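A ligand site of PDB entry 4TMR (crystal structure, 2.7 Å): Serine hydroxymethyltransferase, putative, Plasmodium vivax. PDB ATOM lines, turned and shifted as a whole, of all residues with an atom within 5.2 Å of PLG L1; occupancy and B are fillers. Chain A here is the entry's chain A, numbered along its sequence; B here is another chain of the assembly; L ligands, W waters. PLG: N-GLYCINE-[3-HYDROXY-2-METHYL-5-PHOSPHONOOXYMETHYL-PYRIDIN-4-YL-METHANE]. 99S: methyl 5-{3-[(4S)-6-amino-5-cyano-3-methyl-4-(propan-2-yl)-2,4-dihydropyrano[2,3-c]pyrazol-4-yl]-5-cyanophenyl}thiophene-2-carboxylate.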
ATOM      1  N   ILE A  32     -15.839  -0.779 -34.217  1.00  0.00           N
ATOM      2  CA  ILE A  32     -15.978  -1.165 -32.797  1.00  0.00           C
ATOM      3  C   ILE A  32     -14.693  -1.804 -32.278  1.00  0.00           C
ATOM      4  O   ILE A  32     -14.269  -2.851 -32.765  1.00  0.00           O
ATOM      5  CB  ILE A  32     -17.165  -2.119 -32.556  1.00  0.00           C
ATOM      6  CG1 ILE A  32     -18.435  -1.649 -33.284  1.00  0.00           C
ATOM      7  CG2 ILE A  32     -17.403  -2.287 -31.067  1.00  0.00           C
ATOM      8  CD1 ILE A  32     -19.086  -0.400 -32.721  1.00  0.00           C
ATOM      9  N   SER A  34     -13.907  -3.308 -29.613  1.00  0.00           N
ATOM     10  CA  SER A  34     -14.141  -4.610 -28.992  1.00  0.00           C
ATOM     11  C   SER A  34     -14.523  -5.724 -29.949  1.00  0.00           C
ATOM     12  O   SER A  34     -14.614  -6.871 -29.541  1.00  0.00           O
ATOM     13  CB  SER A  34     -15.223  -4.492 -27.931  1.00  0.00           C
ATOM     14  OG  SER A  34     -16.249  -3.612 -28.313  1.00  0.00           O
ATOM     15  N   SER A 100     -17.786 -15.531 -20.283  1.00  0.00           N
ATOM     16  CA  SER A 100     -17.521 -14.247 -20.912  1.00  0.00           C
ATOM     17  C   SER A 100     -16.716 -13.345 -19.952  1.00  0.00           C
ATOM     18  O   SER A 100     -16.583 -13.633 -18.754  1.00  0.00           O
ATOM     19  CB  SER A 100     -18.846 -13.573 -21.298  1.00  0.00           C
ATOM     20  OG  SER A 100     -18.748 -12.850 -22.537  1.00  0.00           O
ATOM     21  N   GLY A 101     -16.193 -12.233 -20.470  1.00  0.00           N
ATOM     22  CA  GLY A 101     -15.339 -11.361 -19.683  1.00  0.00           C
ATOM     23  C   GLY A 101     -15.969 -10.886 -18.390  1.00  0.00           C
ATOM     24  O   GLY A 101     -15.299 -10.738 -17.387  1.00  0.00           O
ATOM     25  N   SER A 102     -17.269 -10.637 -18.430  1.00  0.00           N
ATOM     26  CA  SER A 102     -17.966 -10.127 -17.254  1.00  0.00           C
ATOM     27  C   SER A 102     -18.064 -11.204 -16.170  1.00  0.00           C
ATOM     28  O   SER A 102     -17.918 -10.900 -14.984  1.00  0.00           O
ATOM     29  CB  SER A 102     -19.345  -9.558 -17.616  1.00  0.00           C
ATOM     30  OG  SER A 102     -19.260  -8.230 -18.149  1.00  0.00           O
ATOM     31  N   ALA A 103     -18.306 -12.450 -16.572  1.00  0.00           N
ATOM     32  CA  ALA A 103     -18.343 -13.552 -15.627  1.00  0.00           C
ATOM     33  C   ALA A 103     -16.974 -13.796 -14.981  1.00  0.00           C
ATOM     34  O   ALA A 103     -16.896 -13.931 -13.763  1.00  0.00           O
ATOM     35  CB  ALA A 103     -18.879 -14.822 -16.295  1.00  0.00           C
ATOM     36  N   ASN A 105     -14.299 -11.699 -14.624  1.00  0.00           N
ATOM     37  CA  ASN A 105     -14.015 -10.650 -13.659  1.00  0.00           C
ATOM     38  C   ASN A 105     -14.768 -10.859 -12.337  1.00  0.00           C
ATOM     39  O   ASN A 105     -14.131 -10.902 -11.288  1.00  0.00           O
ATOM     40  CB  ASN A 105     -14.276  -9.249 -14.207  1.00  0.00           C
ATOM     41  CG  ASN A 105     -13.322  -8.869 -15.339  1.00  0.00           C
ATOM     42  OD1 ASN A 105     -12.707  -9.721 -15.962  1.00  0.00           O
ATOM     43  ND2 ASN A 105     -13.229  -7.576 -15.609  1.00  0.00           N
ATOM     44  N   HIS A 129     -14.345  -0.593 -17.061  1.00  0.00           N
ATOM     45  CA  HIS A 129     -15.473  -1.446 -17.413  1.00  0.00           C
ATOM     46  C   HIS A 129     -16.473  -1.451 -16.318  1.00  0.00           C
ATOM     47  O   HIS A 129     -16.173  -1.076 -15.174  1.00  0.00           O
ATOM     48  CB  HIS A 129     -15.006  -2.872 -17.689  1.00  0.00           C
ATOM     49  CG  HIS A 129     -16.033  -3.714 -18.407  1.00  0.00           C
ATOM     50  ND1 HIS A 129     -16.643  -4.769 -17.822  1.00  0.00           N
ATOM     51  CD2 HIS A 129     -16.593  -3.596 -19.686  1.00  0.00           C
ATOM     52  CE1 HIS A 129     -17.519  -5.309 -18.698  1.00  0.00           C
ATOM     53  NE2 HIS A 129     -17.486  -4.582 -19.828  1.00  0.00           N
ATOM     54  N   THR A 131     -17.746  -4.100 -14.859  1.00  0.00           N
ATOM     55  CA  THR A 131     -17.345  -5.099 -13.876  1.00  0.00           C
ATOM     56  C   THR A 131     -16.170  -4.675 -13.001  1.00  0.00           C
ATOM     57  O   THR A 131     -15.663  -5.470 -12.209  1.00  0.00           O
ATOM     58  CB  THR A 131     -16.922  -6.409 -14.528  1.00  0.00           C
ATOM     59  OG1 THR A 131     -15.938  -6.137 -15.531  1.00  0.00           O
ATOM     60  CG2 THR A 131     -18.105  -7.102 -15.124  1.00  0.00           C
ATOM     61  N   HIS A 132     -15.717  -3.439 -13.130  1.00  0.00           N
ATOM     62  CA  HIS A 132     -14.641  -2.957 -12.297  1.00  0.00           C
ATOM     63  C   HIS A 132     -15.168  -2.178 -11.155  1.00  0.00           C
ATOM     64  O   HIS A 132     -14.467  -1.368 -10.576  1.00  0.00           O
ATOM     65  CB  HIS A 132     -13.657  -2.115 -13.103  1.00  0.00           C
ATOM     66  CG  HIS A 132     -12.952  -2.878 -14.186  1.00  0.00           C
ATOM     67  ND1 HIS A 132     -12.345  -2.269 -15.205  1.00  0.00           N
ATOM     68  CD2 HIS A 132     -12.786  -4.231 -14.389  1.00  0.00           C
ATOM     69  CE1 HIS A 132     -11.798  -3.191 -16.012  1.00  0.00           C
ATOM     70  NE2 HIS A 132     -12.066  -4.394 -15.518  1.00  0.00           N
ATOM     71  N   GLY A 181      -6.289  -2.025 -16.379  1.00  0.00           N
ATOM     72  CA  GLY A 181      -6.649  -2.627 -17.672  1.00  0.00           C
ATOM     73  C   GLY A 181      -8.082  -2.228 -17.990  1.00  0.00           C
ATOM     74  O   GLY A 181      -8.987  -2.472 -17.182  1.00  0.00           O
ATOM     75  N   TYR A 182      -8.301  -1.588 -19.122  1.00  0.00           N
ATOM     76  CA  TYR A 182      -9.543  -0.834 -19.279  1.00  0.00           C
ATOM     77  C   TYR A 182     -10.292  -1.112 -20.544  1.00  0.00           C
ATOM     78  O   TYR A 182      -9.794  -1.830 -21.407  1.00  0.00           O
ATOM     79  CB  TYR A 182      -9.271   0.659 -19.124  1.00  0.00           C
ATOM     80  CG  TYR A 182      -8.342   0.938 -17.960  1.00  0.00           C
ATOM     81  CD1 TYR A 182      -8.723   0.648 -16.641  1.00  0.00           C
ATOM     82  CD2 TYR A 182      -7.082   1.464 -18.176  1.00  0.00           C
ATOM     83  CE1 TYR A 182      -7.855   0.881 -15.587  1.00  0.00           C
ATOM     84  CE2 TYR A 182      -6.213   1.728 -17.131  1.00  0.00           C
ATOM     85  CZ  TYR A 182      -6.612   1.437 -15.838  1.00  0.00           C
ATOM     86  OH  TYR A 182      -5.753   1.699 -14.812  1.00  0.00           O
ATOM     87  N   THR A 183     -11.509  -0.575 -20.651  1.00  0.00           N
ATOM     88  CA  THR A 183     -12.332  -0.849 -21.815  1.00  0.00           C
ATOM     89  C   THR A 183     -12.156   0.154 -22.960  1.00  0.00           C
ATOM     90  O   THR A 183     -12.125  -0.228 -24.120  1.00  0.00           O
ATOM     91  CB  THR A 183     -13.806  -1.153 -21.457  1.00  0.00           C
ATOM     92  OG1 THR A 183     -14.707  -0.159 -21.962  1.00  0.00           O
ATOM     93  CG2 THR A 183     -13.964  -1.257 -20.001  1.00  0.00           C
ATOM     94  N   ASP A 208      -6.928  -6.482 -16.173  1.00  0.00           N
ATOM     95  CA  ASP A 208      -7.878  -6.938 -17.178  1.00  0.00           C
ATOM     96  C   ASP A 208      -7.437  -6.376 -18.511  1.00  0.00           C
ATOM     97  O   ASP A 208      -7.608  -5.196 -18.774  1.00  0.00           O
ATOM     98  CB  ASP A 208      -9.298  -6.476 -16.845  1.00  0.00           C
ATOM     99  CG  ASP A 208     -10.315  -6.903 -17.891  1.00  0.00           C
ATOM    100  OD1 ASP A 208      -9.927  -7.449 -18.946  1.00  0.00           O
ATOM    101  OD2 ASP A 208     -11.528  -6.680 -17.634  1.00  0.00           O
ATOM    102  N   SER A 210      -8.345  -7.309 -21.661  1.00  0.00           N
ATOM    103  CA  SER A 210      -9.283  -7.771 -22.696  1.00  0.00           C
ATOM    104  C   SER A 210      -9.159  -7.023 -24.021  1.00  0.00           C
ATOM    105  O   SER A 210      -9.283  -7.619 -25.077  1.00  0.00           O
ATOM    106  CB  SER A 210     -10.698  -7.682 -22.184  1.00  0.00           C
ATOM    107  OG  SER A 210     -10.872  -8.583 -21.113  1.00  0.00           O
ATOM    108  N   HIS A 211      -8.910  -5.719 -23.959  1.00  0.00           N
ATOM    109  CA  HIS A 211      -8.753  -4.947 -25.177  1.00  0.00           C
ATOM    110  C   HIS A 211      -7.423  -5.109 -25.839  1.00  0.00           C
ATOM    111  O   HIS A 211      -7.330  -5.074 -27.062  1.00  0.00           O
ATOM    112  CB  HIS A 211      -9.133  -3.488 -24.949  1.00  0.00           C
ATOM    113  CG  HIS A 211     -10.581  -3.189 -25.304  1.00  0.00           C
ATOM    114  ND1 HIS A 211     -10.928  -2.623 -26.488  1.00  0.00           N
ATOM    115  CD2 HIS A 211     -11.763  -3.449 -24.625  1.00  0.00           C
ATOM    116  CE1 HIS A 211     -12.263  -2.517 -26.548  1.00  0.00           C
ATOM    117  NE2 HIS A 211     -12.784  -3.017 -25.405  1.00  0.00           N
ATOM    118  N   THR A 234     -10.787 -11.477 -22.187  1.00  0.00           N
ATOM    119  CA  THR A 234     -11.791 -12.047 -23.061  1.00  0.00           C
ATOM    120  C   THR A 234     -11.068 -12.597 -24.275  1.00  0.00           C
ATOM    121  O   THR A 234      -9.944 -12.221 -24.535  1.00  0.00           O
ATOM    122  CB  THR A 234     -12.771 -10.964 -23.501  1.00  0.00           C
ATOM    123  OG1 THR A 234     -12.036  -9.781 -23.863  1.00  0.00           O
ATOM    124  CG2 THR A 234     -13.711 -10.626 -22.388  1.00  0.00           C
ATOM    125  N   HIS A 236     -12.635 -12.856 -27.519  1.00  0.00           N
ATOM    126  CA  HIS A 236     -13.356 -12.483 -28.742  1.00  0.00           C
ATOM    127  C   HIS A 236     -12.956 -11.159 -29.304  1.00  0.00           C
ATOM    128  O   HIS A 236     -13.430 -10.784 -30.380  1.00  0.00           O
ATOM    129  CB  HIS A 236     -14.879 -12.518 -28.518  1.00  0.00           C
ATOM    130  CG  HIS A 236     -15.344 -11.829 -27.250  1.00  0.00           C
ATOM    131  ND1 HIS A 236     -15.234 -12.395 -26.036  1.00  0.00           N
ATOM    132  CD2 HIS A 236     -15.954 -10.596 -27.049  1.00  0.00           C
ATOM    133  CE1 HIS A 236     -15.743 -11.563 -25.106  1.00  0.00           C
ATOM    134  NE2 HIS A 236     -16.169 -10.460 -25.724  1.00  0.00           N
ATOM    135  N   LYS A 237     -12.101 -10.430 -28.611  1.00  0.00           N
ATOM    136  CA  LYS A 237     -11.723  -9.123 -29.119  1.00  0.00           C
ATOM    137  C   LYS A 237     -10.461  -9.169 -30.002  1.00  0.00           C
ATOM    138  O   LYS A 237     -10.450  -9.828 -31.044  1.00  0.00           O
ATOM    139  CB  LYS A 237     -11.581  -8.115 -27.981  1.00  0.00           C
ATOM    140  CG  LYS A 237     -12.844  -7.931 -27.144  1.00  0.00           C
ATOM    141  CD  LYS A 237     -12.613  -6.835 -26.122  1.00  0.00           C
ATOM    142  CE  LYS A 237     -13.830  -6.642 -25.229  1.00  0.00           C
ATOM    143  NZ  LYS A 237     -14.133  -7.789 -24.355  1.00  0.00           N
ATOM    144  N   ARG A 243     -16.331 -16.020 -28.151  1.00  0.00           N
ATOM    145  CA  ARG A 243     -16.748 -15.277 -26.989  1.00  0.00           C
ATOM    146  C   ARG A 243     -16.584 -16.137 -25.762  1.00  0.00           C
ATOM    147  O   ARG A 243     -17.303 -17.123 -25.579  1.00  0.00           O
ATOM    148  CB  ARG A 243     -18.188 -14.813 -27.116  1.00  0.00           C
ATOM    149  CG  ARG A 243     -18.456 -13.969 -28.334  1.00  0.00           C
ATOM    150  CD  ARG A 243     -19.841 -13.343 -28.240  1.00  0.00           C
ATOM    151  NE  ARG A 243     -19.813 -12.146 -27.410  1.00  0.00           N
ATOM    152  CZ  ARG A 243     -19.514 -10.918 -27.858  1.00  0.00           C
ATOM    153  NH1 ARG A 243     -19.216 -10.728 -29.148  1.00  0.00           N
ATOM    154  NH2 ARG A 243     -19.513  -9.898 -27.003  1.00  0.00           N
ATOM    155  N   ARG A 371     -15.669   6.145 -29.921  1.00  0.00           N
ATOM    156  CA  ARG A 371     -14.518   5.310 -29.784  1.00  0.00           C
ATOM    157  C   ARG A 371     -14.407   4.427 -31.005  1.00  0.00           C
ATOM    158  O   ARG A 371     -15.300   3.653 -31.304  1.00  0.00           O
ATOM    159  CB  ARG A 371     -14.652   4.456 -28.532  1.00  0.00           C
ATOM    160  CG  ARG A 371     -13.452   3.578 -28.228  1.00  0.00           C
ATOM    161  CD  ARG A 371     -13.819   2.553 -27.175  1.00  0.00           C
ATOM    162  NE  ARG A 371     -14.670   1.479 -27.681  1.00  0.00           N
ATOM    163  CZ  ARG A 371     -14.957   0.379 -27.003  1.00  0.00           C
ATOM    164  NH1 ARG A 371     -14.466   0.224 -25.790  1.00  0.00           N
ATOM    165  NH2 ARG A 371     -15.736  -0.557 -27.517  1.00  0.00           N
ATOM    166  N   TYR B  54     -21.353  -7.093 -30.941  1.00  0.00           N
ATOM    167  CA  TYR B  54     -21.477  -6.633 -29.576  1.00  0.00           C
ATOM    168  C   TYR B  54     -22.766  -5.836 -29.496  1.00  0.00           C
ATOM    169  O   TYR B  54     -22.896  -4.776 -30.114  1.00  0.00           O
ATOM    170  CB  TYR B  54     -20.308  -5.733 -29.200  1.00  0.00           C
ATOM    171  CG  TYR B  54     -19.538  -6.253 -28.019  1.00  0.00           C
ATOM    172  CD1 TYR B  54     -20.129  -6.314 -26.747  1.00  0.00           C
ATOM    173  CD2 TYR B  54     -18.240  -6.705 -28.176  1.00  0.00           C
ATOM    174  CE1 TYR B  54     -19.422  -6.808 -25.674  1.00  0.00           C
ATOM    175  CE2 TYR B  54     -17.526  -7.200 -27.096  1.00  0.00           C
ATOM    176  CZ  TYR B  54     -18.117  -7.261 -25.854  1.00  0.00           C
ATOM    177  OH  TYR B  54     -17.411  -7.754 -24.811  1.00  0.00           O
ATOM    178  N   GLU B  56     -24.640  -4.976 -26.366  1.00  0.00           N
ATOM    179  CA  GLU B  56     -25.036  -4.750 -24.980  1.00  0.00           C
ATOM    180  C   GLU B  56     -26.301  -3.933 -24.940  1.00  0.00           C
ATOM    181  O   GLU B  56     -26.401  -2.904 -25.600  1.00  0.00           O
ATOM    182  CB  GLU B  56     -23.931  -4.054 -24.198  1.00  0.00           C
ATOM    183  CG  GLU B  56     -22.609  -4.782 -24.334  1.00  0.00           C
ATOM    184  CD  GLU B  56     -21.534  -4.196 -23.478  1.00  0.00           C
ATOM    185  OE1 GLU B  56     -21.626  -4.290 -22.254  1.00  0.00           O
ATOM    186  OE2 GLU B  56     -20.579  -3.632 -24.028  1.00  0.00           O
ATOM    187  N   TYR B  64     -25.243   0.458 -29.046  1.00  0.00           N
ATOM    188  CA  TYR B  64     -24.756   0.665 -30.414  1.00  0.00           C
ATOM    189  C   TYR B  64     -25.861   0.696 -31.461  1.00  0.00           C
ATOM    190  O   TYR B  64     -27.053   0.756 -31.139  1.00  0.00           O
ATOM    191  CB  TYR B  64     -23.707  -0.384 -30.795  1.00  0.00           C
ATOM    192  CG  TYR B  64     -22.662  -0.655 -29.745  1.00  0.00           C
ATOM    193  CD1 TYR B  64     -22.511   0.189 -28.652  1.00  0.00           C
ATOM    194  CD2 TYR B  64     -21.800  -1.750 -29.869  1.00  0.00           C
ATOM    195  CE1 TYR B  64     -21.545  -0.057 -27.706  1.00  0.00           C
ATOM    196  CE2 TYR B  64     -20.814  -2.017 -28.920  1.00  0.00           C
ATOM    197  CZ  TYR B  64     -20.690  -1.164 -27.840  1.00  0.00           C
ATOM    198  OH  TYR B  64     -19.715  -1.408 -26.873  1.00  0.00           O
ATOM    199  N   GLN B 270     -23.978  -9.393 -16.656  1.00  0.00           N
ATOM    200  CA  GLN B 270     -23.361  -9.744 -17.922  1.00  0.00           C
ATOM    201  C   GLN B 270     -22.872  -8.551 -18.710  1.00  0.00           C
ATOM    202  O   GLN B 270     -23.087  -7.417 -18.309  1.00  0.00           O
ATOM    203  CB  GLN B 270     -24.322 -10.588 -18.748  1.00  0.00           C
ATOM    204  CG  GLN B 270     -24.667 -11.918 -18.129  1.00  0.00           C
ATOM    205  CD  GLN B 270     -25.340 -12.873 -19.083  1.00  0.00           C
ATOM    206  OE1 GLN B 270     -25.576 -14.031 -18.742  1.00  0.00           O
ATOM    207  NE2 GLN B 270     -25.654 -12.411 -20.282  1.00  0.00           N
ATOM    208  N   GLY B 271     -22.146  -8.829 -19.792  1.00  0.00           N
ATOM    209  CA  GLY B 271     -21.740  -7.826 -20.787  1.00  0.00           C
ATOM    210  C   GLY B 271     -22.521  -8.071 -22.071  1.00  0.00           C
ATOM    211  O   GLY B 271     -23.750  -8.184 -22.037  1.00  0.00           O
ATOM    212  N   GLY B 272     -21.815  -8.199 -23.192  1.00  0.00           N
ATOM    213  CA  GLY B 272     -22.442  -8.501 -24.481  1.00  0.00           C
ATOM    214  C   GLY B 272     -23.221  -9.805 -24.436  1.00  0.00           C
ATOM    215  O   GLY B 272     -22.806 -10.722 -23.748  1.00  0.00           O
HETATM  216  N1  PLG L   1     -13.627  -6.489 -19.612  1.00  0.00           N
HETATM  217  C2  PLG L   1     -13.244  -5.360 -20.272  1.00  0.00           C
HETATM  218  C2A PLG L   1     -12.100  -4.518 -19.771  1.00  0.00           C
HETATM  219  C3  PLG L   1     -13.924  -4.977 -21.416  1.00  0.00           C
HETATM  220  O3  PLG L   1     -13.596  -3.856 -22.108  1.00  0.00           O
HETATM  221  C4  PLG L   1     -14.981  -5.730 -21.877  1.00  0.00           C
HETATM  222  C4A PLG L   1     -15.724  -5.308 -23.095  1.00  0.00           C
HETATM  223  C5  PLG L   1     -15.345  -6.873 -21.164  1.00  0.00           C
HETATM  224  C6  PLG L   1     -14.651  -7.244 -20.034  1.00  0.00           C
HETATM  225  C5A PLG L   1     -16.475  -7.653 -21.701  1.00  0.00           C
HETATM  226  OP4 PLG L   1     -16.975  -8.866 -21.107  1.00  0.00           O
HETATM  227  P   PLG L   1     -18.079  -9.647 -21.954  1.00  0.00           P
HETATM  228  OP1 PLG L   1     -18.903 -10.251 -20.836  1.00  0.00           O
HETATM  229  OP2 PLG L   1     -18.797  -8.570 -22.719  1.00  0.00           O
HETATM  230  OP3 PLG L   1     -17.272 -10.619 -22.766  1.00  0.00           O
HETATM  231  C   PLG L   1     -16.578  -3.157 -25.168  1.00  0.00           C
HETATM  232  O   PLG L   1     -17.288  -2.770 -26.120  1.00  0.00           O
HETATM  233  OXT PLG L   1     -15.330  -3.012 -25.154  1.00  0.00           O
HETATM  234  CA  PLG L   1     -17.352  -3.819 -24.042  1.00  0.00           C
HETATM  235  N   PLG L   1     -16.529  -4.350 -22.973  1.00  0.00           N
HETATM  236  O31 99S L   2     -25.847   3.794 -16.541  1.00  0.00           O
HETATM  237  C30 99S L   2     -25.723   2.638 -16.933  1.00  0.00           C
HETATM  238  O32 99S L   2     -26.447   1.560 -16.312  1.00  0.00           O
HETATM  239  C33 99S L   2     -27.254   2.082 -15.253  1.00  0.00           C
HETATM  240  C28 99S L   2     -24.834   2.277 -18.053  1.00  0.00           C
HETATM  241  C27 99S L   2     -24.572   1.050 -18.638  1.00  0.00           C
HETATM  242  C26 99S L   2     -23.677   1.143 -19.701  1.00  0.00           C
HETATM  243  S29 99S L   2     -23.972   3.542 -18.842  1.00  0.00           S
HETATM  244  C25 99S L   2     -23.230   2.437 -19.934  1.00  0.00           C
HETATM  245  C21 99S L   2     -22.304   2.969 -20.954  1.00  0.00           C
HETATM  246  C20 99S L   2     -22.557   4.176 -21.567  1.00  0.00           C
HETATM  247  C19 99S L   2     -21.687   4.629 -22.555  1.00  0.00           C
HETATM  248  C23 99S L   2     -21.890   5.771 -23.085  1.00  0.00           C
HETATM  249  N24 99S L   2     -22.073   6.796 -23.586  1.00  0.00           N
HETATM  250  C18 99S L   2     -20.577   3.895 -22.925  1.00  0.00           C
HETATM  251  C22 99S L   2     -21.217   2.207 -21.334  1.00  0.00           C
HETATM  252  C17 99S L   2     -20.342   2.656 -22.328  1.00  0.00           C
HETATM  253  C4  99S L   2     -19.127   1.847 -22.697  1.00  0.00           C
HETATM  254  C14 99S L   2     -18.839   1.790 -24.214  1.00  0.00           C
HETATM  255  C16 99S L   2     -19.952   1.160 -25.050  1.00  0.00           C
HETATM  256  C15 99S L   2     -17.514   1.098 -24.532  1.00  0.00           C
HETATM  257  C3  99S L   2     -18.003   2.620 -22.030  1.00  0.00           C
HETATM  258  C8  99S L   2     -17.833   3.846 -22.311  1.00  0.00           C
HETATM  259  N9  99S L   2     -17.665   4.957 -22.552  1.00  0.00           N
HETATM  260  C2  99S L   2     -17.109   2.075 -21.187  1.00  0.00           C
HETATM  261  N7  99S L   2     -16.021   2.757 -20.810  1.00  0.00           N
HETATM  262  C5  99S L   2     -19.205   0.493 -22.069  1.00  0.00           C
HETATM  263  C10 99S L   2     -20.142  -0.655 -22.194  1.00  0.00           C
HETATM  264  C13 99S L   2     -21.373  -0.758 -23.074  1.00  0.00           C
HETATM  265  N11 99S L   2     -19.718  -1.628 -21.358  1.00  0.00           N
HETATM  266  N12 99S L   2     -18.565  -1.250 -20.638  1.00  0.00           N
HETATM  267  C6  99S L   2     -18.280  -0.020 -21.069  1.00  0.00           C
HETATM  268  O1  99S L   2     -17.238   0.741 -20.667  1.00  0.00           O
HETATM  269  O   HOH W   1     -19.845 -11.193 -24.835  1.00  0.00           O
HETATM  270  O   HOH W   2     -21.306 -11.409 -21.001  1.00  0.00           O
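His 132 touches PLG L1 (CE1 to C2A, 3.998 Å).
Tyr 182 touches PLG L1 (O to C2A, 3.9 Å).
CB of Thr 183 touches O3 of PLG L1, at 2.8 Å.
OG of Ser 210 touches N1 of PLG L1, at 3.8 Å.
CG2 of Thr 234 touches OP3 of PLG L1, at 3.6 Å.
Lys 237 touches PLG L1.
Glu 56 of chain B touches PLG L1 (OE2 to CA, 3.2 Å).
CA of Gly 271 of chain B touches OP2 of PLG L1 (3.6 Å).
20 residues have an atom within 4 Å of PLG L1: Ser 34, Ser 100, Gly 101, Ser 102, His 129, His 132, Tyr 182, Thr 183, Asp 208, Ser 210, His 211, Thr 234, His 236, Lys 237, Arg 371, Tyr 54 of chain B, Glu 56 of chain B, Tyr 64 of chain B, Gly 271 of chain B and Gly 272 of chain B.
The nearest printed residue that does not touch PLG L1 is Asn 105 (4.2 Å).
Water W2 lies within hydrogen-bond range of OP1 of PLG L1, N of Gly 271 of chain B, O of Gly 272 of chain B and OG of Ser 100.
Water W1 lies within hydrogen-bond range of NH2 of Arg 243 (2.5 Å), OG of Ser 100 (3.0 Å), O of Gly 272 of chain B (3.2 Å) and OP3 of PLG L1 (3.4 Å).
A ring nitrogen (NE2) of His 211 is in hydrogen-bond range of an oxygen (OXT) of PLG L1, 2.6 Å away.
The side-chain hydroxyl (OG) of Ser 34 lies within hydrogen-bond range of an oxygen (O) of PLG L1, at 2.6 Å.
OP2 of PLG L1 lies within hydrogen-bond range of OH of Tyr 54 of chain B, at 2.6 Å.
OG of Ser 100 sits at hydrogen-bond distance from OP3 of PLG L1.
An oxygen (O) of PLG L1 lies within hydrogen-bond range of the side-chain hydroxyl of Tyr 64 of chain B (2.9 Å).
The side-chain carboxylate of Asp 208 is in hydrogen-bond range of a nitrogen (N1) of PLG L1.
The backbone NH (N) of Ser 102 sits at hydrogen-bond distance from an oxygen (OP1) of PLG L1, 2.9 Å away.
OG of Ser 102 sits close to OP1 of PLG L1 (3.4 Å).
A ring nitrogen (NE2) of His 236 sits close to an oxygen (OP3) of PLG L1 (3.2 Å).
The backbone NH (N) of Gly 101 sits at hydrogen-bond distance from an oxygen (OP3) of PLG L1, at 3.0 Å.
The guanidinium group (NH2) of Arg 371 lies within salt-bridge range of an oxygen (O) of PLG L1, 3.0 Å away.
The backbone NH of Gly 272 of chain B lies within hydrogen-bond range of an oxygen (OP2) of PLG L1 (3.1 Å).
A ring nitrogen (NE2) of His 129 sits at hydrogen-bond distance from a nitrogen (N) of PLG L1 (3.3 Å).
OG1 of Thr 183 is in hydrogen-bond range of O1 of 99S L2 (3.0 Å).
N11 of 99S L2 sits at hydrogen-bond distance from OE1 of Glu 56 of chain B, at 3.4 Å.
The backbone carbonyl oxygen (O) of Thr 183 sits at hydrogen-bond distance from a ring nitrogen (NE2) of His 211 (3.1 Å).
The backbone carbonyl oxygen (O) of Thr 183 lies within hydrogen-bond range of the guanidinium group (NH1) of Arg 371, 2.9 Å away.
The side-chain carboxylate of Asp 208 is in hydrogen-bond range of a ring nitrogen (NE2) of His 132 (3.2 Å).
The side-chain amide nitrogen of Asn 105 is in hydrogen-bond range of the side-chain carboxylate of Asp 208 (2.8 Å).
The side-chain hydroxyl (OG) of Ser 102 is in hydrogen-bond range of the backbone NH (N) of Gly 271 of chain B (3.4 Å).
The backbone carbonyl oxygen (O) of Gly 101 lies close to the side-chain amide oxygen (OD1) of Asn 105, at 3.1 Å.
ND1 of His 129 is in hydrogen-bond range of OG1 of Thr 131 (2.8 Å).
The backbone NH (N) of Thr 234 lies within hydrogen-bond range of the side-chain hydroxyl (OG) of Ser 210 (3.1 Å).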
